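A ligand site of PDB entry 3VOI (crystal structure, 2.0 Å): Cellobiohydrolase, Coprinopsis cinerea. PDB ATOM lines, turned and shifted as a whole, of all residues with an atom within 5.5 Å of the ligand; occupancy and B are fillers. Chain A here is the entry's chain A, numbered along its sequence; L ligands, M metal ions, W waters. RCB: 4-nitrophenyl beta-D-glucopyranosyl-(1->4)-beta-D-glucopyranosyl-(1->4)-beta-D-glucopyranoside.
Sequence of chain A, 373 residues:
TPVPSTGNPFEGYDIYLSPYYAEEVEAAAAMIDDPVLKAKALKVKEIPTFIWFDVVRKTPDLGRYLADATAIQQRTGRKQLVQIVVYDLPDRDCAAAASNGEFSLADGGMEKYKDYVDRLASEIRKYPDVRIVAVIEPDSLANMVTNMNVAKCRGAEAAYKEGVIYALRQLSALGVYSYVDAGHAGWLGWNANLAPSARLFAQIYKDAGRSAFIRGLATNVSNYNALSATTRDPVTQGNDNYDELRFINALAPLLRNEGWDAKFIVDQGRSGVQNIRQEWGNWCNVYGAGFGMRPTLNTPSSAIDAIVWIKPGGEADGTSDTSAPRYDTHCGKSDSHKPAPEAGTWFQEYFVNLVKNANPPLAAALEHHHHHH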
ATOM      1  N   ASP A  93     -20.372 -26.320   2.600  1.00  0.00           N
ATOM      2  CA  ASP A  93     -19.400 -25.726   1.683  1.00  0.00           C
ATOM      3  C   ASP A  93     -18.023 -25.626   2.337  1.00  0.00           C
ATOM      4  O   ASP A  93     -17.406 -24.549   2.375  1.00  0.00           O
ATOM      5  CB  ASP A  93     -19.895 -24.349   1.233  1.00  0.00           C
ATOM      6  CG  ASP A  93     -19.229 -23.851  -0.024  1.00  0.00           C
ATOM      7  OD1 ASP A  93     -18.821 -24.678  -0.893  1.00  0.00           O
ATOM      8  OD2 ASP A  93     -19.134 -22.617  -0.165  1.00  0.00           O
ATOM      9  N   ALA A  95     -14.925 -26.474   1.985  1.00  0.00           N
ATOM     10  CA  ALA A  95     -13.663 -26.125   1.337  1.00  0.00           C
ATOM     11  C   ALA A  95     -13.677 -24.676   0.855  1.00  0.00           C
ATOM     12  O   ALA A  95     -12.707 -24.209   0.268  1.00  0.00           O
ATOM     13  CB  ALA A  95     -13.390 -27.075   0.184  1.00  0.00           C
ATOM     14  N   ALA A  96     -14.771 -23.968   1.095  1.00  0.00           N
ATOM     15  CA  ALA A  96     -14.940 -22.619   0.584  1.00  0.00           C
ATOM     16  C   ALA A  96     -15.551 -21.672   1.610  1.00  0.00           C
ATOM     17  O   ALA A  96     -16.088 -22.117   2.628  1.00  0.00           O
ATOM     18  CB  ALA A  96     -15.786 -22.622  -0.701  1.00  0.00           C
ATOM     19  N   ASP A 139     -21.883 -30.623  -3.474  1.00  0.00           N
ATOM     20  CA  ASP A 139     -20.507 -30.517  -2.948  1.00  0.00           C
ATOM     21  C   ASP A 139     -20.188 -31.393  -1.755  1.00  0.00           C
ATOM     22  O   ASP A 139     -19.029 -31.722  -1.554  1.00  0.00           O
ATOM     23  CB  ASP A 139     -20.138 -29.064  -2.649  1.00  0.00           C
ATOM     24  CG  ASP A 139     -20.396 -28.151  -3.826  1.00  0.00           C
ATOM     25  OD1 ASP A 139     -20.331 -28.656  -4.975  1.00  0.00           O
ATOM     26  OD2 ASP A 139     -20.682 -26.950  -3.593  1.00  0.00           O
ATOM     27  N   ASN A 143     -16.440 -33.195  -1.425  1.00  0.00           N
ATOM     28  CA  ASN A 143     -15.472 -32.720  -0.430  1.00  0.00           C
ATOM     29  C   ASN A 143     -14.955 -33.829   0.480  1.00  0.00           C
ATOM     30  O   ASN A 143     -13.802 -33.818   0.898  1.00  0.00           O
ATOM     31  CB  ASN A 143     -16.065 -31.585   0.405  1.00  0.00           C
ATOM     32  CG  ASN A 143     -15.970 -30.235  -0.273  1.00  0.00           C
ATOM     33  OD1 ASN A 143     -16.900 -29.430  -0.224  1.00  0.00           O
ATOM     34  ND2 ASN A 143     -14.833 -29.991  -0.919  1.00  0.00           N
ATOM     35  N   THR A 146     -12.185 -35.598  -1.416  1.00  0.00           N
ATOM     36  CA  THR A 146     -11.043 -34.851  -1.917  1.00  0.00           C
ATOM     37  C   THR A 146     -10.366 -33.908  -0.935  1.00  0.00           C
ATOM     38  O   THR A 146      -9.178 -33.602  -1.102  1.00  0.00           O
ATOM     39  CB  THR A 146     -11.438 -34.033  -3.171  1.00  0.00           C
ATOM     40  OG1 THR A 146     -12.494 -33.116  -2.827  1.00  0.00           O
ATOM     41  CG2 THR A 146     -11.906 -34.970  -4.284  1.00  0.00           C
ATOM     42  N   ASN A 147     -11.105 -33.469   0.095  1.00  0.00           N
ATOM     43  CA  ASN A 147     -10.649 -32.362   0.941  1.00  0.00           C
ATOM     44  C   ASN A 147     -10.550 -32.597   2.449  1.00  0.00           C
ATOM     45  O   ASN A 147     -10.701 -31.665   3.238  1.00  0.00           O
ATOM     46  CB  ASN A 147     -11.518 -31.122   0.684  1.00  0.00           C
ATOM     47  CG  ASN A 147     -11.119 -30.369  -0.568  1.00  0.00           C
ATOM     48  OD1 ASN A 147      -9.935 -30.117  -0.809  1.00  0.00           O
ATOM     49  ND2 ASN A 147     -12.098 -29.997  -1.366  1.00  0.00           N
ATOM     50  N   HIS A 184     -18.313 -33.228 -10.303  1.00  0.00           N
ATOM     51  CA  HIS A 184     -18.274 -33.069 -11.769  1.00  0.00           C
ATOM     52  C   HIS A 184     -17.014 -33.708 -12.314  1.00  0.00           C
ATOM     53  O   HIS A 184     -16.180 -34.190 -11.545  1.00  0.00           O
ATOM     54  CB  HIS A 184     -18.401 -31.580 -12.198  1.00  0.00           C
ATOM     55  CG  HIS A 184     -17.299 -30.694 -11.702  1.00  0.00           C
ATOM     56  ND1 HIS A 184     -16.161 -30.437 -12.446  1.00  0.00           N
ATOM     57  CD2 HIS A 184     -17.166 -29.973 -10.564  1.00  0.00           C
ATOM     58  CE1 HIS A 184     -15.376 -29.616 -11.769  1.00  0.00           C
ATOM     59  NE2 HIS A 184     -15.949 -29.330 -10.617  1.00  0.00           N
ATOM     60  N   GLY A 186     -14.274 -32.543 -13.612  1.00  0.00           N
ATOM     61  CA  GLY A 186     -13.013 -31.947 -13.134  1.00  0.00           C
ATOM     62  C   GLY A 186     -12.821 -32.007 -11.631  1.00  0.00           C
ATOM     63  O   GLY A 186     -11.867 -31.426 -11.105  1.00  0.00           O
ATOM     64  N   TRP A 187     -13.710 -32.699 -10.934  1.00  0.00           N
ATOM     65  CA  TRP A 187     -13.572 -32.867  -9.483  1.00  0.00           C
ATOM     66  C   TRP A 187     -13.336 -34.342  -9.175  1.00  0.00           C
ATOM     67  O   TRP A 187     -12.252 -34.731  -8.743  1.00  0.00           O
ATOM     68  CB  TRP A 187     -14.817 -32.349  -8.748  1.00  0.00           C
ATOM     69  CG  TRP A 187     -14.633 -32.092  -7.242  1.00  0.00           C
ATOM     70  CD1 TRP A 187     -13.618 -32.551  -6.443  1.00  0.00           C
ATOM     71  CD2 TRP A 187     -15.520 -31.359  -6.384  1.00  0.00           C
ATOM     72  NE1 TRP A 187     -13.811 -32.129  -5.141  1.00  0.00           N
ATOM     73  CE2 TRP A 187     -14.973 -31.399  -5.087  1.00  0.00           C
ATOM     74  CE3 TRP A 187     -16.729 -30.686  -6.594  1.00  0.00           C
ATOM     75  CZ2 TRP A 187     -15.596 -30.775  -4.002  1.00  0.00           C
ATOM     76  CZ3 TRP A 187     -17.339 -30.059  -5.514  1.00  0.00           C
ATOM     77  CH2 TRP A 187     -16.768 -30.105  -4.235  1.00  0.00           C
ATOM     78  N   TRP A 190     -11.174 -37.322 -12.125  1.00  0.00           N
ATOM     79  CA  TRP A 190      -9.759 -37.689 -12.045  1.00  0.00           C
ATOM     80  C   TRP A 190      -9.600 -39.112 -11.523  1.00  0.00           C
ATOM     81  O   TRP A 190     -10.284 -39.505 -10.600  1.00  0.00           O
ATOM     82  CB  TRP A 190      -9.042 -36.737 -11.093  1.00  0.00           C
ATOM     83  CG  TRP A 190      -8.967 -35.351 -11.602  1.00  0.00           C
ATOM     84  CD1 TRP A 190      -9.771 -34.296 -11.259  1.00  0.00           C
ATOM     85  CD2 TRP A 190      -8.047 -34.852 -12.579  1.00  0.00           C
ATOM     86  NE1 TRP A 190      -9.397 -33.168 -11.953  1.00  0.00           N
ATOM     87  CE2 TRP A 190      -8.340 -33.478 -12.762  1.00  0.00           C
ATOM     88  CE3 TRP A 190      -6.997 -35.425 -13.305  1.00  0.00           C
ATOM     89  CZ2 TRP A 190      -7.614 -32.668 -13.646  1.00  0.00           C
ATOM     90  CZ3 TRP A 190      -6.262 -34.624 -14.173  1.00  0.00           C
ATOM     91  CH2 TRP A 190      -6.581 -33.256 -14.345  1.00  0.00           C
ATOM     92  N   ALA A 192      -7.373 -40.279  -9.618  1.00  0.00           N
ATOM     93  CA  ALA A 192      -7.172 -40.177  -8.172  1.00  0.00           C
ATOM     94  C   ALA A 192      -8.477 -40.359  -7.374  1.00  0.00           C
ATOM     95  O   ALA A 192      -8.441 -40.914  -6.268  1.00  0.00           O
ATOM     96  CB  ALA A 192      -6.509 -38.820  -7.827  1.00  0.00           C
ATOM     97  N   ASN A 193      -9.609 -39.909  -7.937  1.00  0.00           N
ATOM     98  CA  ASN A 193     -10.858 -39.771  -7.172  1.00  0.00           C
ATOM     99  C   ASN A 193     -12.010 -40.710  -7.541  1.00  0.00           C
ATOM    100  O   ASN A 193     -12.933 -40.872  -6.739  1.00  0.00           O
ATOM    101  CB  ASN A 193     -11.337 -38.310  -7.175  1.00  0.00           C
ATOM    102  CG  ASN A 193     -10.327 -37.374  -6.538  1.00  0.00           C
ATOM    103  OD1 ASN A 193      -9.574 -37.774  -5.640  1.00  0.00           O
ATOM    104  ND2 ASN A 193     -10.275 -36.135  -7.011  1.00  0.00           N
ATOM    105  N   VAL A 221     -23.409 -29.653 -10.938  1.00  0.00           N
ATOM    106  CA  VAL A 221     -24.202 -28.662 -10.203  1.00  0.00           C
ATOM    107  C   VAL A 221     -23.385 -27.388  -9.963  1.00  0.00           C
ATOM    108  O   VAL A 221     -22.267 -27.457  -9.431  1.00  0.00           O
ATOM    109  CB  VAL A 221     -24.767 -29.221  -8.872  1.00  0.00           C
ATOM    110  CG1 VAL A 221     -25.628 -28.151  -8.178  1.00  0.00           C
ATOM    111  CG2 VAL A 221     -25.614 -30.478  -9.136  1.00  0.00           C
ATOM    112  N   SER A 222     -23.950 -26.263 -10.394  1.00  0.00           N
ATOM    113  CA  SER A 222     -23.309 -24.927 -10.330  1.00  0.00           C
ATOM    114  C   SER A 222     -21.973 -24.851 -11.057  1.00  0.00           C
ATOM    115  O   SER A 222     -21.169 -23.965 -10.774  1.00  0.00           O
ATOM    116  CB  SER A 222     -23.152 -24.433  -8.891  1.00  0.00           C
ATOM    117  OG  SER A 222     -24.376 -24.579  -8.195  1.00  0.00           O
ATOM    118  N   ASN A 223     -21.730 -25.767 -11.969  1.00  0.00           N
ATOM    119  CA  ASN A 223     -20.496 -25.744 -12.724  1.00  0.00           C
ATOM    120  C   ASN A 223     -20.764 -25.522 -14.210  1.00  0.00           C
ATOM    121  O   ASN A 223     -21.871 -25.174 -14.589  1.00  0.00           O
ATOM    122  CB  ASN A 223     -19.612 -26.963 -12.422  1.00  0.00           C
ATOM    123  CG  ASN A 223     -18.129 -26.656 -12.561  1.00  0.00           C
ATOM    124  OD1 ASN A 223     -17.598 -26.609 -13.692  1.00  0.00           O
ATOM    125  ND2 ASN A 223     -17.448 -26.441 -11.438  1.00  0.00           N
ATOM    126  N   GLY A 238      -4.888 -33.664 -18.993  1.00  0.00           N
ATOM    127  CA  GLY A 238      -4.477 -34.649 -18.006  1.00  0.00           C
ATOM    128  C   GLY A 238      -5.622 -35.515 -17.503  1.00  0.00           C
ATOM    129  O   GLY A 238      -5.378 -36.565 -16.902  1.00  0.00           O
ATOM    130  N   TRP A 280      -9.350 -25.350 -14.101  1.00  0.00           N
ATOM    131  CA  TRP A 280     -10.593 -26.117 -14.063  1.00  0.00           C
ATOM    132  C   TRP A 280     -11.280 -25.934 -12.700  1.00  0.00           C
ATOM    133  O   TRP A 280     -12.491 -25.855 -12.623  1.00  0.00           O
ATOM    134  CB  TRP A 280     -10.310 -27.590 -14.354  1.00  0.00           C
ATOM    135  CG  TRP A 280     -11.515 -28.339 -14.874  1.00  0.00           C
ATOM    136  CD1 TRP A 280     -12.798 -27.891 -14.936  1.00  0.00           C
ATOM    137  CD2 TRP A 280     -11.527 -29.676 -15.396  1.00  0.00           C
ATOM    138  NE1 TRP A 280     -13.616 -28.849 -15.486  1.00  0.00           N
ATOM    139  CE2 TRP A 280     -12.867 -29.959 -15.767  1.00  0.00           C
ATOM    140  CE3 TRP A 280     -10.556 -30.660 -15.589  1.00  0.00           C
ATOM    141  CZ2 TRP A 280     -13.250 -31.188 -16.309  1.00  0.00           C
ATOM    142  CZ3 TRP A 280     -10.940 -31.889 -16.131  1.00  0.00           C
ATOM    143  CH2 TRP A 280     -12.271 -32.141 -16.486  1.00  0.00           C
ATOM    144  N   GLY A 281     -10.474 -25.809 -11.644  1.00  0.00           N
ATOM    145  CA  GLY A 281     -10.989 -25.606 -10.274  1.00  0.00           C
ATOM    146  C   GLY A 281     -11.562 -24.227  -9.956  1.00  0.00           C
ATOM    147  O   GLY A 281     -11.899 -23.965  -8.798  1.00  0.00           O
ATOM    148  N   TRP A 283     -14.561 -21.775 -10.089  1.00  0.00           N
ATOM    149  CA  TRP A 283     -15.990 -22.080 -10.115  1.00  0.00           C
ATOM    150  C   TRP A 283     -16.882 -20.866  -9.855  1.00  0.00           C
ATOM    151  O   TRP A 283     -18.107 -20.930 -10.012  1.00  0.00           O
ATOM    152  CB  TRP A 283     -16.305 -23.161  -9.077  1.00  0.00           C
ATOM    153  CG  TRP A 283     -15.728 -22.817  -7.727  1.00  0.00           C
ATOM    154  CD1 TRP A 283     -14.519 -23.219  -7.231  1.00  0.00           C
ATOM    155  CD2 TRP A 283     -16.310 -21.976  -6.708  1.00  0.00           C
ATOM    156  NE1 TRP A 283     -14.313 -22.702  -5.977  1.00  0.00           N
ATOM    157  CE2 TRP A 283     -15.402 -21.946  -5.628  1.00  0.00           C
ATOM    158  CE3 TRP A 283     -17.524 -21.276  -6.604  1.00  0.00           C
ATOM    159  CZ2 TRP A 283     -15.651 -21.210  -4.459  1.00  0.00           C
ATOM    160  CZ3 TRP A 283     -17.765 -20.543  -5.455  1.00  0.00           C
ATOM    161  CH2 TRP A 283     -16.842 -20.510  -4.394  1.00  0.00           C
HETATM  162  C1A RCB L   1     -15.853 -26.589  -5.535  1.00  0.00           C
HETATM  163  O1A RCB L   1     -14.477 -26.559  -5.902  1.00  0.00           O
HETATM  164  C1B RCB L   1     -11.691 -29.148  -7.660  1.00  0.00           C
HETATM  165  O1B RCB L   1     -11.150 -30.380  -8.140  1.00  0.00           O
HETATM  166  C1C RCB L   1      -7.974 -32.931  -7.576  1.00  0.00           C
HETATM  167  O1C RCB L   1      -6.743 -33.553  -7.198  1.00  0.00           O
HETATM  168  C1D RCB L   1      -5.920 -34.199  -8.068  1.00  0.00           C
HETATM  169  N1D RCB L   1      -3.373 -36.155 -10.760  1.00  0.00           N
HETATM  170  C2A RCB L   1     -16.113 -25.517  -4.470  1.00  0.00           C
HETATM  171  O2A RCB L   1     -15.465 -25.818  -3.218  1.00  0.00           O
HETATM  172  C2B RCB L   1     -13.004 -28.926  -8.417  1.00  0.00           C
HETATM  173  O2B RCB L   1     -12.722 -28.779  -9.817  1.00  0.00           O
HETATM  174  C2C RCB L   1      -8.793 -32.682  -6.320  1.00  0.00           C
HETATM  175  O2C RCB L   1      -9.035 -33.946  -5.700  1.00  0.00           O
HETATM  176  C2D RCB L   1      -6.066 -34.022  -9.441  1.00  0.00           C
HETATM  177  O2D RCB L   1      -2.488 -36.913 -10.378  1.00  0.00           O
HETATM  178  C3A RCB L   1     -17.615 -25.349  -4.218  1.00  0.00           C
HETATM  179  O3A RCB L   1     -17.775 -24.219  -3.345  1.00  0.00           O
HETATM  180  C3B RCB L   1     -13.705 -27.677  -7.898  1.00  0.00           C
HETATM  181  O3B RCB L   1     -14.957 -27.508  -8.578  1.00  0.00           O
HETATM  182  C3C RCB L   1     -10.102 -32.000  -6.720  1.00  0.00           C
HETATM  183  O3C RCB L   1     -10.811 -31.567  -5.551  1.00  0.00           O
HETATM  184  C3D RCB L   1      -5.224 -34.670 -10.322  1.00  0.00           C
HETATM  185  O3D RCB L   1      -3.453 -35.888 -11.951  1.00  0.00           O
HETATM  186  C4A RCB L   1     -18.345 -25.137  -5.561  1.00  0.00           C
HETATM  187  O4A RCB L   1     -19.766 -25.003  -5.393  1.00  0.00           O
HETATM  188  C4B RCB L   1     -13.941 -27.786  -6.391  1.00  0.00           C
HETATM  189  C4C RCB L   1      -9.885 -30.782  -7.623  1.00  0.00           C
HETATM  190  C4D RCB L   1      -4.221 -35.521  -9.844  1.00  0.00           C
HETATM  191  C5A RCB L   1     -18.044 -26.288  -6.517  1.00  0.00           C
HETATM  192  O5A RCB L   1     -16.624 -26.309  -6.716  1.00  0.00           O
HETATM  193  C5B RCB L   1     -12.617 -28.076  -5.698  1.00  0.00           C
HETATM  194  O5B RCB L   1     -11.957 -29.215  -6.254  1.00  0.00           O
HETATM  195  C5C RCB L   1      -8.932 -31.125  -8.780  1.00  0.00           C
HETATM  196  O5C RCB L   1      -7.736 -31.685  -8.234  1.00  0.00           O
HETATM  197  C5D RCB L   1      -4.077 -35.710  -8.465  1.00  0.00           C
HETATM  198  C6A RCB L   1     -18.768 -26.122  -7.867  1.00  0.00           C
HETATM  199  O6A RCB L   1     -18.428 -27.212  -8.738  1.00  0.00           O
HETATM  200  C6B RCB L   1     -12.835 -28.334  -4.208  1.00  0.00           C
HETATM  201  O6B RCB L   1     -11.570 -28.252  -3.568  1.00  0.00           O
HETATM  202  C6C RCB L   1      -8.579 -29.936  -9.675  1.00  0.00           C
HETATM  203  O6C RCB L   1      -8.065 -30.453 -10.920  1.00  0.00           O
HETATM  204  C6D RCB L   1      -4.931 -35.053  -7.570  1.00  0.00           C
HETATM  205 MG    MG M   1     -22.830 -22.374  -5.022  1.00  0.00          MG
HETATM  206 MG    MG M   2      -4.955 -38.507 -16.494  1.00  0.00          MG
HETATM  207  O   HOH W   1     -19.447 -22.184  -3.046  1.00  0.00           O
HETATM  208  O   HOH W   2     -10.915 -25.580  -3.758  1.00  0.00           O
HETATM  209  O   HOH W   3     -21.260 -23.095  -6.203  1.00  0.00           O
HETATM  210  O   HOH W   4     -13.063 -24.256  -3.255  1.00  0.00           O
HETATM  211  O   HOH W   5      -5.766 -30.046  -6.538  1.00  0.00           O
HETATM  212  O   HOH W   6     -16.581 -26.464  -0.823  1.00  0.00           O
HETATM  213  O   HOH W   7     -14.560 -25.791 -10.990  1.00  0.00           O
HETATM  214  O   HOH W   8     -20.184 -29.280  -8.961  1.00  0.00           O
HETATM  215  O   HOH W   9      -7.909 -34.154  -3.276  1.00  0.00           O
HETATM  216  O   HOH W  10     -21.809 -23.427  -3.515  1.00  0.00           O
HETATM  217  O   HOH W  11      -9.089 -30.618  -3.424  1.00  0.00           O
HETATM  218  O   HOH W  12      -8.953 -27.076  -7.218  1.00  0.00           O
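An oxygen (O6C) of the ligand is in hydrogen-bond range of the indole nitrogen (NE1) of Trp 190 (3.2 Å). O6A of the ligand sits at hydrogen-bond distance from ND2 of Asn 223 (3.0 Å). The side-chain amide nitrogen (ND2) of Asn 193 is in hydrogen-bond range of an oxygen (O2C) of the ligand. O of Gly 186 sits at hydrogen-bond distance from O2B of the ligand. A ring nitrogen (NE2) of His 184 sits at hydrogen-bond distance from an oxygen (O3B) of the ligand, at 2.9 Å. O6B of the ligand is in hydrogen-bond range of ND2 of Asn 147, at 2.9 Å. The side-chain carboxylate (OD1) of Asp 93 is in hydrogen-bond range of an oxygen (O3A) of the ligand. O3C of the ligand sits at hydrogen-bond distance from NE1 of Trp 187 (3.1 Å). An oxygen (O4A) of the ligand sits at hydrogen-bond distance from the side-chain carboxylate of Asp 139 (2.8 Å).
NE2 of His 184 sits at hydrogen-bond distance from ND2 of Asn 223, 3.4 Å away. ND2 of Asn 147 sits close to ND2 of Asn 143, at 2.8 Å. OD1 of Asn 143 lies close to O of Asp 139, at 3.4 Å. The indole nitrogen (NE1) of Trp 187 is in hydrogen-bond range of the side-chain hydroxyl (OG1) of Thr 146, 2.8 Å away. ND1 of His 184 lies within hydrogen-bond range of N of Gly 186, 3.1 Å away. The side-chain hydroxyl (OG1) of Thr 146 lies within hydrogen-bond range of the side-chain amide nitrogen (ND2) of Asn 147, 3.5 Å away. The indole nitrogen (NE1) of Trp 190 lies within hydrogen-bond range of the backbone carbonyl oxygen (O) of Gly 186, 3.1 Å away. The side-chain amide nitrogen (ND2) of Asn 193 sits at hydrogen-bond distance from the backbone carbonyl oxygen (O) of Trp 187 (3.0 Å).
Residues that only touch the ligand: Ala 96 (3.7 Å), Thr 146 (3.4 Å), Ala 192 (3.999 Å), Val 221 (3.9 Å), Gly 281 (3.6 Å) and Trp 283 (3.6 Å). Hydrophobic or aromatic side chains that line the ligand: Ala 96, His 184, Trp 187, Trp 190, Ala 192 and Trp 283. Of the 20 residues printed, 15 come within 4 Å of the ligand.
Water W1 lies within hydrogen-bond range of an oxygen (O3A) of the ligand (2.7 Å) and the side-chain carboxylate of Asp 93 (2.9 Å). Water W9 bridges O of Thr 146 and O2C of the ligand. Water W6 lies within hydrogen-bond range of an oxygen (O2A) of the ligand (2.7 Å), the side-chain carboxylate of Asp 93 (2.9 Å), the side-chain amide oxygen of Asn 143 (3.0 Å) and the backbone NH of Ala 95 (3.3 Å). Water W8 lies within hydrogen-bond range of an oxygen (O6A) of the ligand (2.7 Å) and the backbone carbonyl oxygen of Val 221 (2.8 Å). Water W11 lies within hydrogen-bond range of OD1 of Asn 147 (2.8 Å) and O3C of the ligand (2.9 Å). Water W7 lies within hydrogen-bond range of O of Trp 280 (2.6 Å), O3B of the ligand (3.0 Å) and ND2 of Asn 223 (3.0 Å).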
